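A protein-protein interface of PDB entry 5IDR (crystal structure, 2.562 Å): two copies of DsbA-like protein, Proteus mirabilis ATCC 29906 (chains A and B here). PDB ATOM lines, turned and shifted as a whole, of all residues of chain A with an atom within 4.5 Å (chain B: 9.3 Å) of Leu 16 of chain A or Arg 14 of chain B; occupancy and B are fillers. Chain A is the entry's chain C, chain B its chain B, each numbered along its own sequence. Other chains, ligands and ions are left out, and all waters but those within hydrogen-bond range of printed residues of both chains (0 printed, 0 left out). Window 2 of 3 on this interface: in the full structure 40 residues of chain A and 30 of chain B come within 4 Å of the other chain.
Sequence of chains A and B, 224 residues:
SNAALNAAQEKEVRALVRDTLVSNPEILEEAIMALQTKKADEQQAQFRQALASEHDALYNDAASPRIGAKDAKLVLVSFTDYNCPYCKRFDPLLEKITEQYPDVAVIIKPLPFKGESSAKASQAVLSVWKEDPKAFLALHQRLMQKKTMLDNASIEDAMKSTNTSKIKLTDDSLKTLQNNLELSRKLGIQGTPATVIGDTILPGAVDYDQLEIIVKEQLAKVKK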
ATOM      1  N   GLU A  12      18.633  10.475 -14.699  1.00  0.00           N
ATOM      2  CA  GLU A  12      19.804  10.665 -13.855  1.00  0.00           C
ATOM      3  C   GLU A  12      19.695  11.960 -13.077  1.00  0.00           C
ATOM      4  O   GLU A  12      20.073  12.018 -11.906  1.00  0.00           O
ATOM      5  CB  GLU A  12      21.082  10.654 -14.701  1.00  0.00           C
ATOM      6  CG  GLU A  12      21.292   9.348 -15.461  1.00  0.00           C
ATOM      7  CD  GLU A  12      21.057   8.119 -14.591  1.00  0.00           C
ATOM      8  OE1 GLU A  12      21.614   8.065 -13.472  1.00  0.00           O
ATOM      9  OE2 GLU A  12      20.301   7.218 -15.021  1.00  0.00           O
ATOM     10  N   VAL A  13      19.170  12.991 -13.730  1.00  0.00           N
ATOM     11  CA  VAL A  13      18.977  14.278 -13.082  1.00  0.00           C
ATOM     12  C   VAL A  13      18.083  14.086 -11.863  1.00  0.00           C
ATOM     13  O   VAL A  13      18.375  14.601 -10.785  1.00  0.00           O
ATOM     14  CB  VAL A  13      18.372  15.320 -14.055  1.00  0.00           C
ATOM     15  CG1 VAL A  13      17.788  16.525 -13.309  1.00  0.00           C
ATOM     16  CG2 VAL A  13      19.430  15.783 -15.033  1.00  0.00           C
ATOM     17  N   ARG A  14      17.012  13.317 -12.029  1.00  0.00           N
ATOM     18  CA  ARG A  14      16.099  13.044 -10.931  1.00  0.00           C
ATOM     19  C   ARG A  14      16.809  12.378  -9.761  1.00  0.00           C
ATOM     20  O   ARG A  14      16.557  12.709  -8.604  1.00  0.00           O
ATOM     21  CB  ARG A  14      14.948  12.165 -11.407  1.00  0.00           C
ATOM     22  CG  ARG A  14      14.014  12.876 -12.351  1.00  0.00           C
ATOM     23  CD  ARG A  14      12.826  12.009 -12.738  1.00  0.00           C
ATOM     24  NE  ARG A  14      11.946  12.714 -13.667  1.00  0.00           N
ATOM     25  CZ  ARG A  14      11.020  13.595 -13.302  1.00  0.00           C
ATOM     26  NH1 ARG A  14      10.834  13.887 -12.020  1.00  0.00           N
ATOM     27  NH2 ARG A  14      10.277  14.189 -14.228  1.00  0.00           N
ATOM     28  N   ALA A  15      17.702  11.444 -10.067  1.00  0.00           N
ATOM     29  CA  ALA A  15      18.423  10.711  -9.034  1.00  0.00           C
ATOM     30  C   ALA A  15      19.541  11.565  -8.441  1.00  0.00           C
ATOM     31  O   ALA A  15      19.970  11.352  -7.303  1.00  0.00           O
ATOM     32  CB  ALA A  15      18.982   9.434  -9.598  1.00  0.00           C
ATOM     33  N   LEU A  16      20.010  12.535  -9.221  1.00  0.00           N
ATOM     34  CA  LEU A  16      21.031  13.465  -8.745  1.00  0.00           C
ATOM     35  C   LEU A  16      20.443  14.460  -7.749  1.00  0.00           C
ATOM     36  O   LEU A  16      21.100  14.821  -6.776  1.00  0.00           O
ATOM     37  CB  LEU A  16      21.676  14.206  -9.919  1.00  0.00           C
ATOM     38  CG  LEU A  16      22.774  13.455 -10.676  1.00  0.00           C
ATOM     39  CD1 LEU A  16      23.159  14.215 -11.933  1.00  0.00           C
ATOM     40  CD2 LEU A  16      23.995  13.237  -9.791  1.00  0.00           C
ATOM     41  N   VAL A  17      19.209  14.896  -8.006  1.00  0.00           N
ATOM     42  CA  VAL A  17      18.485  15.795  -7.110  1.00  0.00           C
ATOM     43  C   VAL A  17      18.416  15.182  -5.715  1.00  0.00           C
ATOM     44  O   VAL A  17      18.687  15.851  -4.713  1.00  0.00           O
ATOM     45  CB  VAL A  17      17.056  16.080  -7.637  1.00  0.00           C
ATOM     46  CG1 VAL A  17      16.148  16.646  -6.540  1.00  0.00           C
ATOM     47  CG2 VAL A  17      17.102  17.026  -8.826  1.00  0.00           C
ATOM     48  N   ARG A  18      18.066  13.903  -5.651  1.00  0.00           N
ATOM     49  CA  ARG A  18      18.014  13.203  -4.374  1.00  0.00           C
ATOM     50  C   ARG A  18      19.409  13.051  -3.762  1.00  0.00           C
ATOM     51  O   ARG A  18      19.629  13.414  -2.617  1.00  0.00           O
ATOM     52  CB  ARG A  18      17.362  11.830  -4.543  1.00  0.00           C
ATOM     53  CG  ARG A  18      17.489  10.917  -3.330  1.00  0.00           C
ATOM     54  CD  ARG A  18      16.779   9.607  -3.584  1.00  0.00           C
ATOM     55  NE  ARG A  18      17.040   8.621  -2.539  1.00  0.00           N
ATOM     56  CZ  ARG A  18      16.511   7.400  -2.515  1.00  0.00           C
ATOM     57  NH1 ARG A  18      15.682   7.010  -3.478  1.00  0.00           N
ATOM     58  NH2 ARG A  18      16.809   6.563  -1.528  1.00  0.00           N
ATOM     59  N   ASP A  19      20.351  12.515  -4.525  1.00  0.00           N
ATOM     60  CA  ASP A  19      21.655  12.188  -3.971  1.00  0.00           C
ATOM     61  C   ASP A  19      22.428  13.431  -3.560  1.00  0.00           C
ATOM     62  O   ASP A  19      23.205  13.404  -2.610  1.00  0.00           O
ATOM     63  CB  ASP A  19      22.487  11.387  -4.972  1.00  0.00           C
ATOM     64  CG  ASP A  19      23.859  11.042  -4.428  1.00  0.00           C
ATOM     65  OD1 ASP A  19      23.988   9.976  -3.780  1.00  0.00           O
ATOM     66  OD2 ASP A  19      24.801  11.847  -4.628  1.00  0.00           O
ATOM     67  N   THR A  20      22.226  14.518  -4.290  1.00  0.00           N
ATOM     68  CA  THR A  20      22.889  15.766  -3.968  1.00  0.00           C
ATOM     69  C   THR A  20      22.409  16.275  -2.612  1.00  0.00           C
ATOM     70  O   THR A  20      23.218  16.719  -1.794  1.00  0.00           O
ATOM     71  CB  THR A  20      22.639  16.830  -5.059  1.00  0.00           C
ATOM     72  OG1 THR A  20      23.311  16.444  -6.260  1.00  0.00           O
ATOM     73  CG2 THR A  20      23.155  18.194  -4.640  1.00  0.00           C
ATOM     74  N   ALA B   4      24.496   7.006 -18.960  1.00  0.00           N
ATOM     75  CA  ALA B   4      25.136   8.072 -18.208  1.00  0.00           C
ATOM     76  C   ALA B   4      24.877   9.450 -18.828  1.00  0.00           C
ATOM     77  O   ALA B   4      23.998   9.616 -19.678  1.00  0.00           O
ATOM     78  CB  ALA B   4      26.644   7.802 -18.100  1.00  0.00           C
ATOM     79  N   LEU B   5      25.636  10.436 -18.359  1.00  0.00           N
ATOM     80  CA  LEU B   5      25.687  11.763 -18.964  1.00  0.00           C
ATOM     81  C   LEU B   5      27.018  12.399 -18.590  1.00  0.00           C
ATOM     82  O   LEU B   5      27.556  12.114 -17.518  1.00  0.00           O
ATOM     83  CB  LEU B   5      24.509  12.646 -18.523  1.00  0.00           C
ATOM     84  CG  LEU B   5      23.987  12.708 -17.081  1.00  0.00           C
ATOM     85  CD1 LEU B   5      24.923  12.064 -16.074  1.00  0.00           C
ATOM     86  CD2 LEU B   5      23.724  14.153 -16.705  1.00  0.00           C
ATOM     87  N   ASN B   6      27.544  13.228 -19.494  1.00  0.00           N
ATOM     88  CA  ASN B   6      28.868  13.844 -19.362  1.00  0.00           C
ATOM     89  C   ASN B   6      29.296  14.070 -17.928  1.00  0.00           C
ATOM     90  O   ASN B   6      28.617  14.766 -17.177  1.00  0.00           O
ATOM     91  CB  ASN B   6      28.891  15.182 -20.096  1.00  0.00           C
ATOM     92  CG  ASN B   6      29.381  15.070 -21.525  1.00  0.00           C
ATOM     93  OD1 ASN B   6      29.363  13.995 -22.126  1.00  0.00           O
ATOM     94  ND2 ASN B   6      29.823  16.193 -22.080  1.00  0.00           N
ATOM     95  N   ALA B   7      30.420  13.473 -17.551  1.00  0.00           N
ATOM     96  CA  ALA B   7      30.938  13.582 -16.190  1.00  0.00           C
ATOM     97  C   ALA B   7      31.023  15.040 -15.719  1.00  0.00           C
ATOM     98  O   ALA B   7      31.008  15.310 -14.515  1.00  0.00           O
ATOM     99  CB  ALA B   7      32.301  12.919 -16.104  1.00  0.00           C
ATOM    100  N   ALA B   8      31.095  15.968 -16.672  1.00  0.00           N
ATOM    101  CA  ALA B   8      31.105  17.403 -16.375  1.00  0.00           C
ATOM    102  C   ALA B   8      29.685  17.938 -16.215  1.00  0.00           C
ATOM    103  O   ALA B   8      29.431  18.830 -15.402  1.00  0.00           O
ATOM    104  CB  ALA B   8      31.833  18.167 -17.471  1.00  0.00           C
ATOM    105  N   GLN B   9      28.764  17.397 -17.008  1.00  0.00           N
ATOM    106  CA  GLN B   9      27.354  17.749 -16.895  1.00  0.00           C
ATOM    107  C   GLN B   9      26.789  17.280 -15.565  1.00  0.00           C
ATOM    108  O   GLN B   9      25.919  17.932 -14.995  1.00  0.00           O
ATOM    109  CB  GLN B   9      26.537  17.133 -18.028  1.00  0.00           C
ATOM    110  CG  GLN B   9      26.822  17.686 -19.404  1.00  0.00           C
ATOM    111  CD  GLN B   9      25.974  17.008 -20.454  1.00  0.00           C
ATOM    112  OE1 GLN B   9      25.579  15.848 -20.293  1.00  0.00           O
ATOM    113  NE2 GLN B   9      25.685  17.722 -21.536  1.00  0.00           N
ATOM    114  N   GLU B  10      27.272  16.131 -15.093  1.00  0.00           N
ATOM    115  CA  GLU B  10      26.844  15.583 -13.809  1.00  0.00           C
ATOM    116  C   GLU B  10      27.059  16.593 -12.690  1.00  0.00           C
ATOM    117  O   GLU B  10      26.161  16.834 -11.881  1.00  0.00           O
ATOM    118  CB  GLU B  10      27.598  14.286 -13.490  1.00  0.00           C
ATOM    119  CG  GLU B  10      27.380  13.756 -12.063  1.00  0.00           C
ATOM    120  CD  GLU B  10      28.016  12.389 -11.828  1.00  0.00           C
ATOM    121  OE1 GLU B  10      27.844  11.491 -12.683  1.00  0.00           O
ATOM    122  OE2 GLU B  10      28.687  12.212 -10.785  1.00  0.00           O
ATOM    123  N   LYS B  11      28.244  17.194 -12.648  1.00  0.00           N
ATOM    124  CA  LYS B  11      28.552  18.107 -11.565  1.00  0.00           C
ATOM    125  C   LYS B  11      27.822  19.438 -11.731  1.00  0.00           C
ATOM    126  O   LYS B  11      27.597  20.141 -10.744  1.00  0.00           O
ATOM    127  CB  LYS B  11      30.059  18.347 -11.455  1.00  0.00           C
ATOM    128  CG  LYS B  11      30.424  19.009 -10.137  1.00  0.00           C
ATOM    129  CD  LYS B  11      31.905  19.270  -9.975  1.00  0.00           C
ATOM    130  CE  LYS B  11      32.172  19.927  -8.632  1.00  0.00           C
ATOM    131  NZ  LYS B  11      31.339  21.147  -8.431  1.00  0.00           N
ATOM    132  N   GLU B  12      27.442  19.790 -12.957  1.00  0.00           N
ATOM    133  CA  GLU B  12      26.694  21.030 -13.158  1.00  0.00           C
ATOM    134  C   GLU B  12      25.235  20.857 -12.731  1.00  0.00           C
ATOM    135  O   GLU B  12      24.575  21.823 -12.347  1.00  0.00           O
ATOM    136  CB  GLU B  12      26.759  21.501 -14.610  1.00  0.00           C
ATOM    137  CG  GLU B  12      26.026  22.834 -14.817  1.00  0.00           C
ATOM    138  CD  GLU B  12      26.221  23.426 -16.198  1.00  0.00           C
ATOM    139  OE1 GLU B  12      27.165  23.006 -16.902  1.00  0.00           O
ATOM    140  OE2 GLU B  12      25.426  24.317 -16.575  1.00  0.00           O
ATOM    141  N   VAL B  13      24.731  19.630 -12.794  1.00  0.00           N
ATOM    142  CA  VAL B  13      23.376  19.359 -12.332  1.00  0.00           C
ATOM    143  C   VAL B  13      23.358  19.451 -10.815  1.00  0.00           C
ATOM    144  O   VAL B  13      22.413  19.984 -10.236  1.00  0.00           O
ATOM    145  CB  VAL B  13      22.868  17.977 -12.800  1.00  0.00           C
ATOM    146  CG1 VAL B  13      21.549  17.617 -12.132  1.00  0.00           C
ATOM    147  CG2 VAL B  13      22.680  17.981 -14.292  1.00  0.00           C
ATOM    148  N   ARG B  14      24.418  18.952 -10.181  1.00  0.00           N
ATOM    149  CA  ARG B  14      24.537  18.997  -8.724  1.00  0.00           C
ATOM    150  C   ARG B  14      24.511  20.442  -8.229  1.00  0.00           C
ATOM    151  O   ARG B  14      23.898  20.748  -7.208  1.00  0.00           O
ATOM    152  CB  ARG B  14      25.818  18.294  -8.258  1.00  0.00           C
ATOM    153  CG  ARG B  14      25.794  16.772  -8.422  1.00  0.00           C
ATOM    154  CD  ARG B  14      27.006  16.100  -7.778  1.00  0.00           C
ATOM    155  NE  ARG B  14      27.000  14.645  -7.934  1.00  0.00           N
ATOM    156  CZ  ARG B  14      26.416  13.789  -7.092  1.00  0.00           C
ATOM    157  NH1 ARG B  14      25.777  14.229  -6.017  1.00  0.00           N
ATOM    158  NH2 ARG B  14      26.471  12.482  -7.326  1.00  0.00           N
ATOM    159  N   ALA B  15      25.157  21.335  -8.966  1.00  0.00           N
ATOM    160  CA  ALA B  15      25.165  22.750  -8.609  1.00  0.00           C
ATOM    161  C   ALA B  15      23.802  23.392  -8.831  1.00  0.00           C
ATOM    162  O   ALA B  15      23.412  24.293  -8.079  1.00  0.00           O
ATOM    163  CB  ALA B  15      26.203  23.484  -9.405  1.00  0.00           C
ATOM    164  N   LEU B  16      23.092  22.943  -9.868  1.00  0.00           N
ATOM    165  CA  LEU B  16      21.787  23.506 -10.191  1.00  0.00           C
ATOM    166  C   LEU B  16      20.769  23.102  -9.132  1.00  0.00           C
ATOM    167  O   LEU B  16      19.829  23.843  -8.854  1.00  0.00           O
ATOM    168  CB  LEU B  16      21.328  23.065 -11.582  1.00  0.00           C
ATOM    169  CG  LEU B  16      22.051  23.763 -12.738  1.00  0.00           C
ATOM    170  CD1 LEU B  16      21.836  23.019 -14.036  1.00  0.00           C
ATOM    171  CD2 LEU B  16      21.568  25.188 -12.880  1.00  0.00           C
ATOM    172  N   VAL B  17      20.969  21.933  -8.530  1.00  0.00           N
ATOM    173  CA  VAL B  17      20.150  21.506  -7.399  1.00  0.00           C
ATOM    174  C   VAL B  17      20.282  22.509  -6.249  1.00  0.00           C
ATOM    175  O   VAL B  17      19.295  22.875  -5.604  1.00  0.00           O
ATOM    176  CB  VAL B  17      20.556  20.092  -6.914  1.00  0.00           C
ATOM    177  CG1 VAL B  17      19.889  19.751  -5.583  1.00  0.00           C
ATOM    178  CG2 VAL B  17      20.201  19.045  -7.956  1.00  0.00           C
ATOM    179  N   ARG B  18      21.512  22.951  -6.009  1.00  0.00           N
ATOM    180  CA  ARG B  18      21.816  23.882  -4.932  1.00  0.00           C
ATOM    181  C   ARG B  18      21.291  25.287  -5.234  1.00  0.00           C
ATOM    182  O   ARG B  18      20.608  25.895  -4.404  1.00  0.00           O
ATOM    183  CB  ARG B  18      23.328  23.915  -4.700  1.00  0.00           C
ATOM    184  CG  ARG B  18      23.802  24.791  -3.550  1.00  0.00           C
ATOM    185  CD  ARG B  18      25.324  24.839  -3.524  1.00  0.00           C
ATOM    186  NE  ARG B  18      25.875  24.876  -2.166  1.00  0.00           N
ATOM    187  CZ  ARG B  18      26.629  23.917  -1.619  1.00  0.00           C
ATOM    188  NH1 ARG B  18      26.950  22.812  -2.295  1.00  0.00           N
ATOM    189  NH2 ARG B  18      27.073  24.065  -0.377  1.00  0.00           N
ATOM    190  N   ASP B  19      21.601  25.798  -6.424  1.00  0.00           N
ATOM    191  CA  ASP B  19      21.231  27.160  -6.780  1.00  0.00           C
ATOM    192  C   ASP B  19      19.728  27.274  -6.946  1.00  0.00           C
ATOM    193  O   ASP B  19      19.153  28.317  -6.660  1.00  0.00           O
ATOM    194  CB  ASP B  19      21.939  27.605  -8.066  1.00  0.00           C
ATOM    195  CG  ASP B  19      21.704  29.079  -8.393  1.00  0.00           C
ATOM    196  OD1 ASP B  19      22.012  29.939  -7.540  1.00  0.00           O
ATOM    197  OD2 ASP B  19      21.207  29.381  -9.501  1.00  0.00           O
ATOM    198  N   THR B  20      19.088  26.204  -7.404  1.00  0.00           N
ATOM    199  CA  THR B  20      17.649  26.242  -7.658  1.00  0.00           C
ATOM    200  C   THR B  20      16.854  26.307  -6.365  1.00  0.00           C
ATOM    201  O   THR B  20      15.904  27.082  -6.248  1.00  0.00           O
ATOM    202  CB  THR B  20      17.170  25.015  -8.456  1.00  0.00           C
ATOM    203  OG1 THR B  20      17.859  24.961  -9.710  1.00  0.00           O
ATOM    204  CG2 THR B  20      15.661  25.083  -8.713  1.00  0.00           C
ATOM    205  N   LEU B  21      17.226  25.475  -5.401  1.00  0.00           N
ATOM    206  CA  LEU B  21      16.512  25.444  -4.136  1.00  0.00           C
ATOM    207  C   LEU B  21      16.693  26.719  -3.329  1.00  0.00           C
ATOM    208  O   LEU B  21      15.722  27.278  -2.832  1.00  0.00           O
ATOM    209  CB  LEU B  21      16.964  24.259  -3.298  1.00  0.00           C
ATOM    210  CG  LEU B  21      16.083  23.032  -3.442  1.00  0.00           C
ATOM    211  CD1 LEU B  21      16.744  21.891  -2.722  1.00  0.00           C
ATOM    212  CD2 LEU B  21      14.677  23.286  -2.896  1.00  0.00           C
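Printed residues of chain B within 4 Å of Val 13 of chain A: Val 13.
No residue of chain B comes within 4 Å of Ala 15 of chain A.
Arg 18 of chain A touches none of the printed residues of chain B.
Asp 19 of chain A touches just one residue of chain B: Arg 14 (2.9 Å).
Printed residues of chain B within 4 Å of Thr 20 of chain A: Arg 14 (3.3 Å) and Val 17 (3.7 Å).
Of the printed residues of chain A, Glu 10 of chain B touches Leu 16.
Of the printed residues of chain A, Val 13 of chain B touches Val 13 (3.99 Å) and Leu 16 (3.8 Å).
Arg 14 of chain B touches just these residues of chain A: Leu 16, Asp 19 and Thr 20.
Of the printed residues of chain A, Val 17 of chain B touches Val 17 (3.8 Å) and Thr 20 (3.7 Å).
Leu 21 of chain B touches none of the printed residues of chain A.
The nearest printed residue of chain B that does not touch Leu 16 of chain A is Val 17 of chain B (4.5 Å).
The nearest printed residue of chain A that does not touch Arg 14 of chain B is Ala 15 of chain A (6.6 Å).
The nearest printed residue of chain A that does not touch Glu 10 of chain B is Thr 20 of chain A (6.3 Å).
Printed residues of chain A that touch a printed residue of chain B: Val 13, Leu 16, Val 17, Asp 19 and Thr 20.
Hydrophobic or aromatic side chains of chain A that line the printed part of chain B: Val 13, Leu 16 and Val 17.
Hydrophobic or aromatic side chains of chain B that line the printed part of chain A: Val 13 and Val 17.
Among the printed residues, Asp or Glu carboxylates within 4 Å of a Lys or Arg side-chain nitrogen of the other chain: Asp 19 of chain A with Arg 14 of chain B (2.9 Å).
The backbone carbonyl oxygen (O) of Leu 16 of chain A is in hydrogen-bond range of the side-chain hydroxyl (OG1) of Thr 20 of chain A, at 2.8 Å.
The guanidinium group of Arg 14 of chain B lies within salt-bridge range of the side-chain carboxylate of Asp 19 of chain A (2.9 Å).
OG1 of Thr 20 of chain A sits close to NH1 of Arg 14 of chain B, at 3.3 Å.
Val 13 of chain B touches Val 13 of chain A.
Glu 10 of chain B touches Leu 16 of chain A (O to CD1, 3.98 Å).
CD1 of Leu 16 of chain A touches CG1 of Val 13 of chain B (3.8 Å).
Leu 16 of chain A touches Arg 14 of chain B.
CA of Val 17 of chain A touches CG2 of Val 17 of chain B, at 3.8 Å.
Thr 20 of chain A touches Val 17 of chain B (CG2 to CG1, 3.7 Å).
Val 13 of chain A touches its own counterpart, Val 13 of chain B.
Val 17 of chain B touches its own counterpart, Val 17 of chain A.
Asp 19 of chain A touches Arg 14 of chain B, but with the chains exchanged Arg 14 of chain A does not touch Asp 19 of chain B (14.2 Å).
Thr 20 of chain A touches Val 17 of chain B, but with the chains exchanged Val 17 of chain A does not touch Thr 20 of chain B (8.0 Å).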
